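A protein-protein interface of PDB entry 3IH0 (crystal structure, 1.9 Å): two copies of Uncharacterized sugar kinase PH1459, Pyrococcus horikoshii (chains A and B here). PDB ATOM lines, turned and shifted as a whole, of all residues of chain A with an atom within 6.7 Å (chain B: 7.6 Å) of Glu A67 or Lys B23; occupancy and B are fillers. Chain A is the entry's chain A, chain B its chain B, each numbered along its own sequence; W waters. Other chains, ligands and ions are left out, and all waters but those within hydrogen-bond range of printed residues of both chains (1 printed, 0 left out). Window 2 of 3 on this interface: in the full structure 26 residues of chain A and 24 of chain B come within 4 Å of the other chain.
The backbone carbonyl oxygen of Lys B23 is in hydrogen-bond range of the side-chain amino group of Lys A30 (2.8 Å).
The backbone carbonyl oxygen (O) of Val B25 is in hydrogen-bond range of the side-chain amino group (NZ) of Lys A30.
The backbone NH (N) of Lys A30 sits at hydrogen-bond distance from the backbone carbonyl oxygen (O) of Arg B26, 2.8 Å away.
The side-chain carboxylate of Glu A67 is in salt-bridge range of the side-chain amino group of Lys B23 (2.8 Å).
The side-chain carboxylate of Asp B24 lies within salt-bridge range of the side-chain amino group of Lys B23, at 2.6 Å.
Among the printed residues, pairs that only touch across the chains: Tyr A64 with Lys B23 (3.3 Å), Phe A61 with Leu B22 (3.7 Å), Pro A60 with Lys B23 (3.7 Å) and Lys A30 with Leu B22 (3.9 Å).
Of the printed residues of chain B, Glu A67 touches Lys B23 (2.8 Å).
Of chain A, only Lys A30 (2.8 Å), Pro A60 (3.7 Å), Tyr A64 (3.3 Å) and Glu A67 (2.8 Å) come within 4 Å of Lys B23.
Printed residues of chain A within 4 Å of Arg B26: Lys A30.
Printed residues of chain A within 4 Å of Val B25: Lys A30.
Printed residues of chain B within 4 Å of Lys A30: Leu B22, Lys B23, Val B25 and Arg B26.
Of the printed residues of chain A, Leu B22 touches Lys A30 (3.9 Å) and Phe A61 (3.7 Å).
Printed residues of chain B within 4 Å of Phe A61: Leu B22.
The nearest residue of chain A that does not touch Lys B23 is Glu A63 (4.1 Å).
Of the 15 printed residues of chain A, 5 touch a printed residue of chain B.
Printed residues of chain A that touch a printed residue of chain B: Lys A30, Pro A60, Phe A61, Tyr A64 and Glu A67.
Hydrophobic or aromatic side chains of chain A within 4 Å of the printed part of chain B: Phe A61 and Tyr A64.
No position is printed for both chains.
Of the 8 pairs that touch across the chains among the printed residues, none has its exchanged pair printed and touching as well.
Water W1 lies within hydrogen-bond range of O of Lys A30 (2.9 Å) and O of Arg B26 (3.3 Å).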
ATOM      1  N   LYS A  30      24.141 -36.520  -4.725  1.00  0.00           N
ATOM      2  CA  LYS A  30      23.890 -35.831  -3.471  1.00  0.00           C
ATOM      3  C   LYS A  30      22.446 -35.362  -3.321  1.00  0.00           C
ATOM      4  O   LYS A  30      21.860 -34.797  -4.237  1.00  0.00           O
ATOM      5  CB  LYS A  30      24.888 -34.673  -3.356  1.00  0.00           C
ATOM      6  CG  LYS A  30      24.421 -33.415  -2.674  1.00  0.00           C
ATOM      7  CD  LYS A  30      25.597 -32.432  -2.542  1.00  0.00           C
ATOM      8  CE  LYS A  30      25.137 -30.976  -2.462  1.00  0.00           C
ATOM      9  NZ  LYS A  30      24.573 -30.471  -3.755  1.00  0.00           N
ATOM     10  N   PRO A  60      29.869 -25.710   2.724  1.00  0.00           N
ATOM     11  CA  PRO A  60      28.947 -25.758   1.587  1.00  0.00           C
ATOM     12  C   PRO A  60      27.745 -26.705   1.733  1.00  0.00           C
ATOM     13  O   PRO A  60      26.630 -26.367   1.324  1.00  0.00           O
ATOM     14  CB  PRO A  60      29.860 -26.142   0.434  1.00  0.00           C
ATOM     15  CG  PRO A  60      31.141 -25.476   0.810  1.00  0.00           C
ATOM     16  CD  PRO A  60      31.267 -25.796   2.264  1.00  0.00           C
ATOM     17  N   PHE A  61      27.957 -27.882   2.312  1.00  0.00           N
ATOM     18  CA  PHE A  61      26.844 -28.820   2.463  1.00  0.00           C
ATOM     19  C   PHE A  61      25.844 -28.369   3.518  1.00  0.00           C
ATOM     20  O   PHE A  61      24.654 -28.662   3.410  1.00  0.00           O
ATOM     21  CB  PHE A  61      27.357 -30.227   2.774  1.00  0.00           C
ATOM     22  CG  PHE A  61      28.042 -30.887   1.600  1.00  0.00           C
ATOM     23  CD1 PHE A  61      27.903 -30.368   0.315  1.00  0.00           C
ATOM     24  CD2 PHE A  61      28.808 -32.034   1.781  1.00  0.00           C
ATOM     25  CE1 PHE A  61      28.517 -30.975  -0.773  1.00  0.00           C
ATOM     26  CE2 PHE A  61      29.429 -32.655   0.698  1.00  0.00           C
ATOM     27  CZ  PHE A  61      29.283 -32.126  -0.580  1.00  0.00           C
ATOM     28  N   GLY A  62      26.322 -27.652   4.531  1.00  0.00           N
ATOM     29  CA  GLY A  62      25.410 -27.156   5.557  1.00  0.00           C
ATOM     30  C   GLY A  62      24.507 -26.106   4.931  1.00  0.00           C
ATOM     31  O   GLY A  62      23.301 -26.038   5.200  1.00  0.00           O
ATOM     32  N   GLU A  63      25.102 -25.280   4.081  1.00  0.00           N
ATOM     33  CA  GLU A  63      24.378 -24.224   3.388  1.00  0.00           C
ATOM     34  C   GLU A  63      23.377 -24.824   2.418  1.00  0.00           C
ATOM     35  O   GLU A  63      22.281 -24.307   2.251  1.00  0.00           O
ATOM     36  CB  GLU A  63      25.358 -23.349   2.610  1.00  0.00           C
ATOM     37  CG  GLU A  63      26.240 -22.472   3.473  1.00  0.00           C
ATOM     38  CD  GLU A  63      27.521 -22.056   2.754  1.00  0.00           C
ATOM     39  OE1 GLU A  63      27.466 -21.834   1.522  1.00  0.00           O
ATOM     40  OE2 GLU A  63      28.582 -21.948   3.418  1.00  0.00           O
ATOM     41  N   TYR A  64      23.767 -25.914   1.769  1.00  0.00           N
ATOM     42  CA  TYR A  64      22.909 -26.593   0.807  1.00  0.00           C
ATOM     43  C   TYR A  64      21.648 -27.099   1.491  1.00  0.00           C
ATOM     44  O   TYR A  64      20.540 -26.910   0.988  1.00  0.00           O
ATOM     45  CB  TYR A  64      23.665 -27.763   0.171  1.00  0.00           C
ATOM     46  CG  TYR A  64      22.807 -28.759  -0.581  1.00  0.00           C
ATOM     47  CD1 TYR A  64      22.230 -28.431  -1.804  1.00  0.00           C
ATOM     48  CD2 TYR A  64      22.573 -30.034  -0.065  1.00  0.00           C
ATOM     49  CE1 TYR A  64      21.441 -29.342  -2.497  1.00  0.00           C
ATOM     50  CE2 TYR A  64      21.787 -30.959  -0.750  1.00  0.00           C
ATOM     51  CZ  TYR A  64      21.221 -30.602  -1.970  1.00  0.00           C
ATOM     52  OH  TYR A  64      20.431 -31.489  -2.674  1.00  0.00           O
ATOM     53  N   LEU A  65      21.820 -27.741   2.637  1.00  0.00           N
ATOM     54  CA  LEU A  65      20.684 -28.286   3.360  1.00  0.00           C
ATOM     55  C   LEU A  65      19.755 -27.181   3.832  1.00  0.00           C
ATOM     56  O   LEU A  65      18.544 -27.265   3.654  1.00  0.00           O
ATOM     57  CB  LEU A  65      21.170 -29.130   4.534  1.00  0.00           C
ATOM     58  CG  LEU A  65      21.909 -30.397   4.090  1.00  0.00           C
ATOM     59  CD1 LEU A  65      22.564 -31.062   5.276  1.00  0.00           C
ATOM     60  CD2 LEU A  65      20.934 -31.345   3.404  1.00  0.00           C
ATOM     61  N   ILE A  66      20.310 -26.138   4.434  1.00  0.00           N
ATOM     62  CA  ILE A  66      19.466 -25.040   4.889  1.00  0.00           C
ATOM     63  C   ILE A  66      18.710 -24.435   3.699  1.00  0.00           C
ATOM     64  O   ILE A  66      17.513 -24.182   3.793  1.00  0.00           O
ATOM     65  CB  ILE A  66      20.297 -23.961   5.603  1.00  0.00           C
ATOM     66  CG1 ILE A  66      20.981 -24.574   6.827  1.00  0.00           C
ATOM     67  CG2 ILE A  66      19.393 -22.799   6.036  1.00  0.00           C
ATOM     68  CD1 ILE A  66      22.106 -23.740   7.391  1.00  0.00           C
ATOM     69  N   GLU A  67      19.385 -24.214   2.571  1.00  0.00           N
ATOM     70  CA  GLU A  67      18.696 -23.652   1.407  1.00  0.00           C
ATOM     71  C   GLU A  67      17.555 -24.570   0.971  1.00  0.00           C
ATOM     72  O   GLU A  67      16.427 -24.123   0.762  1.00  0.00           O
ATOM     73  CB  GLU A  67      19.648 -23.458   0.222  1.00  0.00           C
ATOM     74  CG  GLU A  67      20.810 -22.520   0.483  1.00  0.00           C
ATOM     75  CD  GLU A  67      21.674 -22.288  -0.753  1.00  0.00           C
ATOM     76  OE1 GLU A  67      21.798 -23.215  -1.592  1.00  0.00           O
ATOM     77  OE2 GLU A  67      22.245 -21.183  -0.873  1.00  0.00           O
ATOM     78  N   GLU A  68      17.842 -25.859   0.834  1.00  0.00           N
ATOM     79  CA  GLU A  68      16.810 -26.796   0.410  1.00  0.00           C
ATOM     80  C   GLU A  68      15.625 -26.837   1.370  1.00  0.00           C
ATOM     81  O   GLU A  68      14.475 -26.932   0.938  1.00  0.00           O
ATOM     82  CB  GLU A  68      17.396 -28.199   0.248  1.00  0.00           C
ATOM     83  CG  GLU A  68      18.430 -28.300  -0.852  1.00  0.00           C
ATOM     84  CD  GLU A  68      17.884 -27.853  -2.195  1.00  0.00           C
ATOM     85  OE1 GLU A  68      16.944 -28.496  -2.704  1.00  0.00           O
ATOM     86  OE2 GLU A  68      18.389 -26.844  -2.734  1.00  0.00           O
ATOM     87  N   LEU A  69      15.893 -26.755   2.666  1.00  0.00           N
ATOM     88  CA  LEU A  69      14.805 -26.788   3.629  1.00  0.00           C
ATOM     89  C   LEU A  69      13.957 -25.537   3.491  1.00  0.00           C
ATOM     90  O   LEU A  69      12.731 -25.593   3.573  1.00  0.00           O
ATOM     91  CB  LEU A  69      15.349 -26.900   5.049  1.00  0.00           C
ATOM     92  CG  LEU A  69      15.814 -28.313   5.398  1.00  0.00           C
ATOM     93  CD1 LEU A  69      16.614 -28.295   6.684  1.00  0.00           C
ATOM     94  CD2 LEU A  69      14.618 -29.230   5.515  1.00  0.00           C
ATOM     95  N   SER A  70      14.620 -24.412   3.249  1.00  0.00           N
ATOM     96  CA  SER A  70      13.918 -23.141   3.098  1.00  0.00           C
ATOM     97  C   SER A  70      13.035 -23.121   1.864  1.00  0.00           C
ATOM     98  O   SER A  70      11.990 -22.468   1.869  1.00  0.00           O
ATOM     99  CB  SER A  70      14.917 -21.982   3.052  1.00  0.00           C
ATOM    100  OG  SER A  70      15.674 -21.942   4.249  1.00  0.00           O
ATOM    101  N   LYS A  71      13.445 -23.825   0.807  1.00  0.00           N
ATOM    102  CA  LYS A  71      12.641 -23.877  -0.406  1.00  0.00           C
ATOM    103  C   LYS A  71      11.358 -24.636  -0.110  1.00  0.00           C
ATOM    104  O   LYS A  71      10.357 -24.462  -0.805  1.00  0.00           O
ATOM    105  CB  LYS A  71      13.369 -24.598  -1.540  1.00  0.00           C
ATOM    106  CG  LYS A  71      14.597 -23.895  -2.081  1.00  0.00           C
ATOM    107  CD  LYS A  71      15.217 -24.722  -3.201  1.00  0.00           C
ATOM    108  CE  LYS A  71      16.482 -24.081  -3.743  1.00  0.00           C
ATOM    109  NZ  LYS A  71      17.157 -24.964  -4.743  1.00  0.00           N
ATOM    110  N   GLU A  72      11.398 -25.500   0.899  1.00  0.00           N
ATOM    111  CA  GLU A  72      10.225 -26.292   1.281  1.00  0.00           C
ATOM    112  C   GLU A  72       9.435 -25.615   2.398  1.00  0.00           C
ATOM    113  O   GLU A  72       8.518 -26.204   2.976  1.00  0.00           O
ATOM    114  CB  GLU A  72      10.651 -27.692   1.737  1.00  0.00           C
ATOM    115  CG  GLU A  72      11.175 -28.597   0.623  1.00  0.00           C
ATOM    116  CD  GLU A  72      10.103 -28.985  -0.396  1.00  0.00           C
ATOM    117  OE1 GLU A  72       8.905 -28.966  -0.047  1.00  0.00           O
ATOM    118  OE2 GLU A  72      10.455 -29.334  -1.542  1.00  0.00           O
ATOM    119  N   THR A  76      14.003 -22.907   9.583  1.00  0.00           N
ATOM    120  CA  THR A  76      15.363 -23.332   9.900  1.00  0.00           C
ATOM    121  C   THR A  76      16.066 -22.528  10.986  1.00  0.00           C
ATOM    122  O   THR A  76      17.260 -22.713  11.205  1.00  0.00           O
ATOM    123  CB  THR A  76      16.266 -23.302   8.660  1.00  0.00           C
ATOM    124  OG1 THR A  76      16.358 -21.960   8.167  1.00  0.00           O
ATOM    125  CG2 THR A  76      15.715 -24.215   7.578  1.00  0.00           C
ATOM    126  N   SER B  16      33.747 -33.729  -8.225  1.00  0.00           N
ATOM    127  CA  SER B  16      32.562 -33.205  -8.875  1.00  0.00           C
ATOM    128  C   SER B  16      32.597 -33.571 -10.356  1.00  0.00           C
ATOM    129  O   SER B  16      33.629 -33.425 -11.007  1.00  0.00           O
ATOM    130  CB  SER B  16      32.507 -31.686  -8.699  1.00  0.00           C
ATOM    131  OG  SER B  16      32.515 -31.352  -7.318  1.00  0.00           O
ATOM    132  N   GLY B  20      30.286 -25.886 -11.075  1.00  0.00           N
ATOM    133  CA  GLY B  20      29.530 -25.204 -10.038  1.00  0.00           C
ATOM    134  C   GLY B  20      30.144 -25.351  -8.662  1.00  0.00           C
ATOM    135  O   GLY B  20      30.993 -26.216  -8.447  1.00  0.00           O
ATOM    136  N   ASP B  21      29.722 -24.500  -7.730  1.00  0.00           N
ATOM    137  CA  ASP B  21      30.213 -24.542  -6.353  1.00  0.00           C
ATOM    138  C   ASP B  21      29.790 -25.890  -5.766  1.00  0.00           C
ATOM    139  O   ASP B  21      28.773 -26.456  -6.177  1.00  0.00           O
ATOM    140  CB  ASP B  21      29.594 -23.397  -5.547  1.00  0.00           C
ATOM    141  CG  ASP B  21      29.910 -22.014  -6.138  1.00  0.00           C
ATOM    142  OD1 ASP B  21      29.011 -21.142  -6.146  1.00  0.00           O
ATOM    143  OD2 ASP B  21      31.060 -21.793  -6.584  1.00  0.00           O
ATOM    144  N   LEU B  22      30.561 -26.412  -4.817  1.00  0.00           N
ATOM    145  CA  LEU B  22      30.235 -27.700  -4.216  1.00  0.00           C
ATOM    146  C   LEU B  22      28.786 -27.751  -3.740  1.00  0.00           C
ATOM    147  O   LEU B  22      28.148 -28.794  -3.788  1.00  0.00           O
ATOM    148  CB  LEU B  22      31.174 -28.007  -3.049  1.00  0.00           C
ATOM    149  CG  LEU B  22      32.574 -28.444  -3.472  1.00  0.00           C
ATOM    150  CD1 LEU B  22      33.480 -28.501  -2.267  1.00  0.00           C
ATOM    151  CD2 LEU B  22      32.493 -29.797  -4.157  1.00  0.00           C
ATOM    152  N   LYS B  23      28.267 -26.615  -3.289  1.00  0.00           N
ATOM    153  CA  LYS B  23      26.893 -26.544  -2.817  1.00  0.00           C
ATOM    154  C   LYS B  23      25.892 -27.022  -3.876  1.00  0.00           C
ATOM    155  O   LYS B  23      24.881 -27.650  -3.553  1.00  0.00           O
ATOM    156  CB  LYS B  23      26.567 -25.100  -2.420  1.00  0.00           C
ATOM    157  CG  LYS B  23      25.188 -24.919  -1.808  1.00  0.00           C
ATOM    158  CD  LYS B  23      24.943 -23.465  -1.435  1.00  0.00           C
ATOM    159  CE  LYS B  23      24.907 -22.575  -2.667  1.00  0.00           C
ATOM    160  NZ  LYS B  23      23.764 -22.898  -3.570  1.00  0.00           N
ATOM    161  N   ASP B  24      26.169 -26.735  -5.144  1.00  0.00           N
ATOM    162  CA  ASP B  24      25.245 -27.125  -6.200  1.00  0.00           C
ATOM    163  C   ASP B  24      25.642 -28.335  -7.046  1.00  0.00           C
ATOM    164  O   ASP B  24      24.953 -28.653  -8.022  1.00  0.00           O
ATOM    165  CB  ASP B  24      24.990 -25.942  -7.134  1.00  0.00           C
ATOM    166  CG  ASP B  24      24.799 -24.641  -6.381  1.00  0.00           C
ATOM    167  OD1 ASP B  24      23.881 -24.575  -5.540  1.00  0.00           O
ATOM    168  OD2 ASP B  24      25.568 -23.687  -6.632  1.00  0.00           O
ATOM    169  N   VAL B  25      26.751 -28.990  -6.713  1.00  0.00           N
ATOM    170  CA  VAL B  25      27.163 -30.157  -7.472  1.00  0.00           C
ATOM    171  C   VAL B  25      26.303 -31.340  -7.049  1.00  0.00           C
ATOM    172  O   VAL B  25      26.163 -31.642  -5.862  1.00  0.00           O
ATOM    173  CB  VAL B  25      28.634 -30.486  -7.248  1.00  0.00           C
ATOM    174  CG1 VAL B  25      28.947 -31.850  -7.822  1.00  0.00           C
ATOM    175  CG2 VAL B  25      29.495 -29.420  -7.908  1.00  0.00           C
ATOM    176  N   ARG B  26      25.742 -32.014  -8.046  1.00  0.00           N
ATOM    177  CA  ARG B  26      24.845 -33.126  -7.809  1.00  0.00           C
ATOM    178  C   ARG B  26      25.499 -34.491  -7.877  1.00  0.00           C
ATOM    179  O   ARG B  26      25.182 -35.368  -7.080  1.00  0.00           O
ATOM    180  CB  ARG B  26      23.702 -33.072  -8.823  1.00  0.00           C
ATOM    181  CG  ARG B  26      22.993 -31.723  -8.880  1.00  0.00           C
ATOM    182  CD  ARG B  26      21.952 -31.683  -9.995  1.00  0.00           C
ATOM    183  NE  ARG B  26      22.552 -31.794 -11.323  1.00  0.00           N
ATOM    184  CZ  ARG B  26      21.858 -31.796 -12.459  1.00  0.00           C
ATOM    185  NH1 ARG B  26      20.535 -31.693 -12.433  1.00  0.00           N
ATOM    186  NH2 ARG B  26      22.485 -31.903 -13.628  1.00  0.00           N
ATOM    187  N   PHE B  28      29.037 -36.953  -8.032  1.00  0.00           N
ATOM    188  CA  PHE B  28      30.444 -37.092  -7.636  1.00  0.00           C
ATOM    189  C   PHE B  28      31.023 -38.450  -8.055  1.00  0.00           C
ATOM    190  O   PHE B  28      30.319 -39.461  -8.040  1.00  0.00           O
ATOM    191  CB  PHE B  28      30.582 -36.970  -6.118  1.00  0.00           C
ATOM    192  CG  PHE B  28      30.255 -35.615  -5.573  1.00  0.00           C
ATOM    193  CD1 PHE B  28      31.239 -34.648  -5.450  1.00  0.00           C
ATOM    194  CD2 PHE B  28      28.953 -35.298  -5.198  1.00  0.00           C
ATOM    195  CE1 PHE B  28      30.944 -33.395  -4.933  1.00  0.00           C
ATOM    196  CE2 PHE B  28      28.642 -34.047  -4.678  1.00  0.00           C
ATOM    197  CZ  PHE B  28      29.634 -33.088  -4.556  1.00  0.00           C
ATOM    198  N   SER B 100      37.825 -25.699  -5.592  1.00  0.00           N
ATOM    199  CA  SER B 100      37.568 -25.720  -4.162  1.00  0.00           C
ATOM    200  C   SER B 100      37.455 -27.136  -3.619  1.00  0.00           C
ATOM    201  O   SER B 100      37.384 -28.102  -4.380  1.00  0.00           O
ATOM    202  CB  SER B 100      36.278 -24.967  -3.857  1.00  0.00           C
ATOM    203  OG  SER B 100      35.178 -25.606  -4.477  1.00  0.00           O
HETATM  204  O   HOH W   1      21.960 -34.828  -7.178  1.00  0.00           O
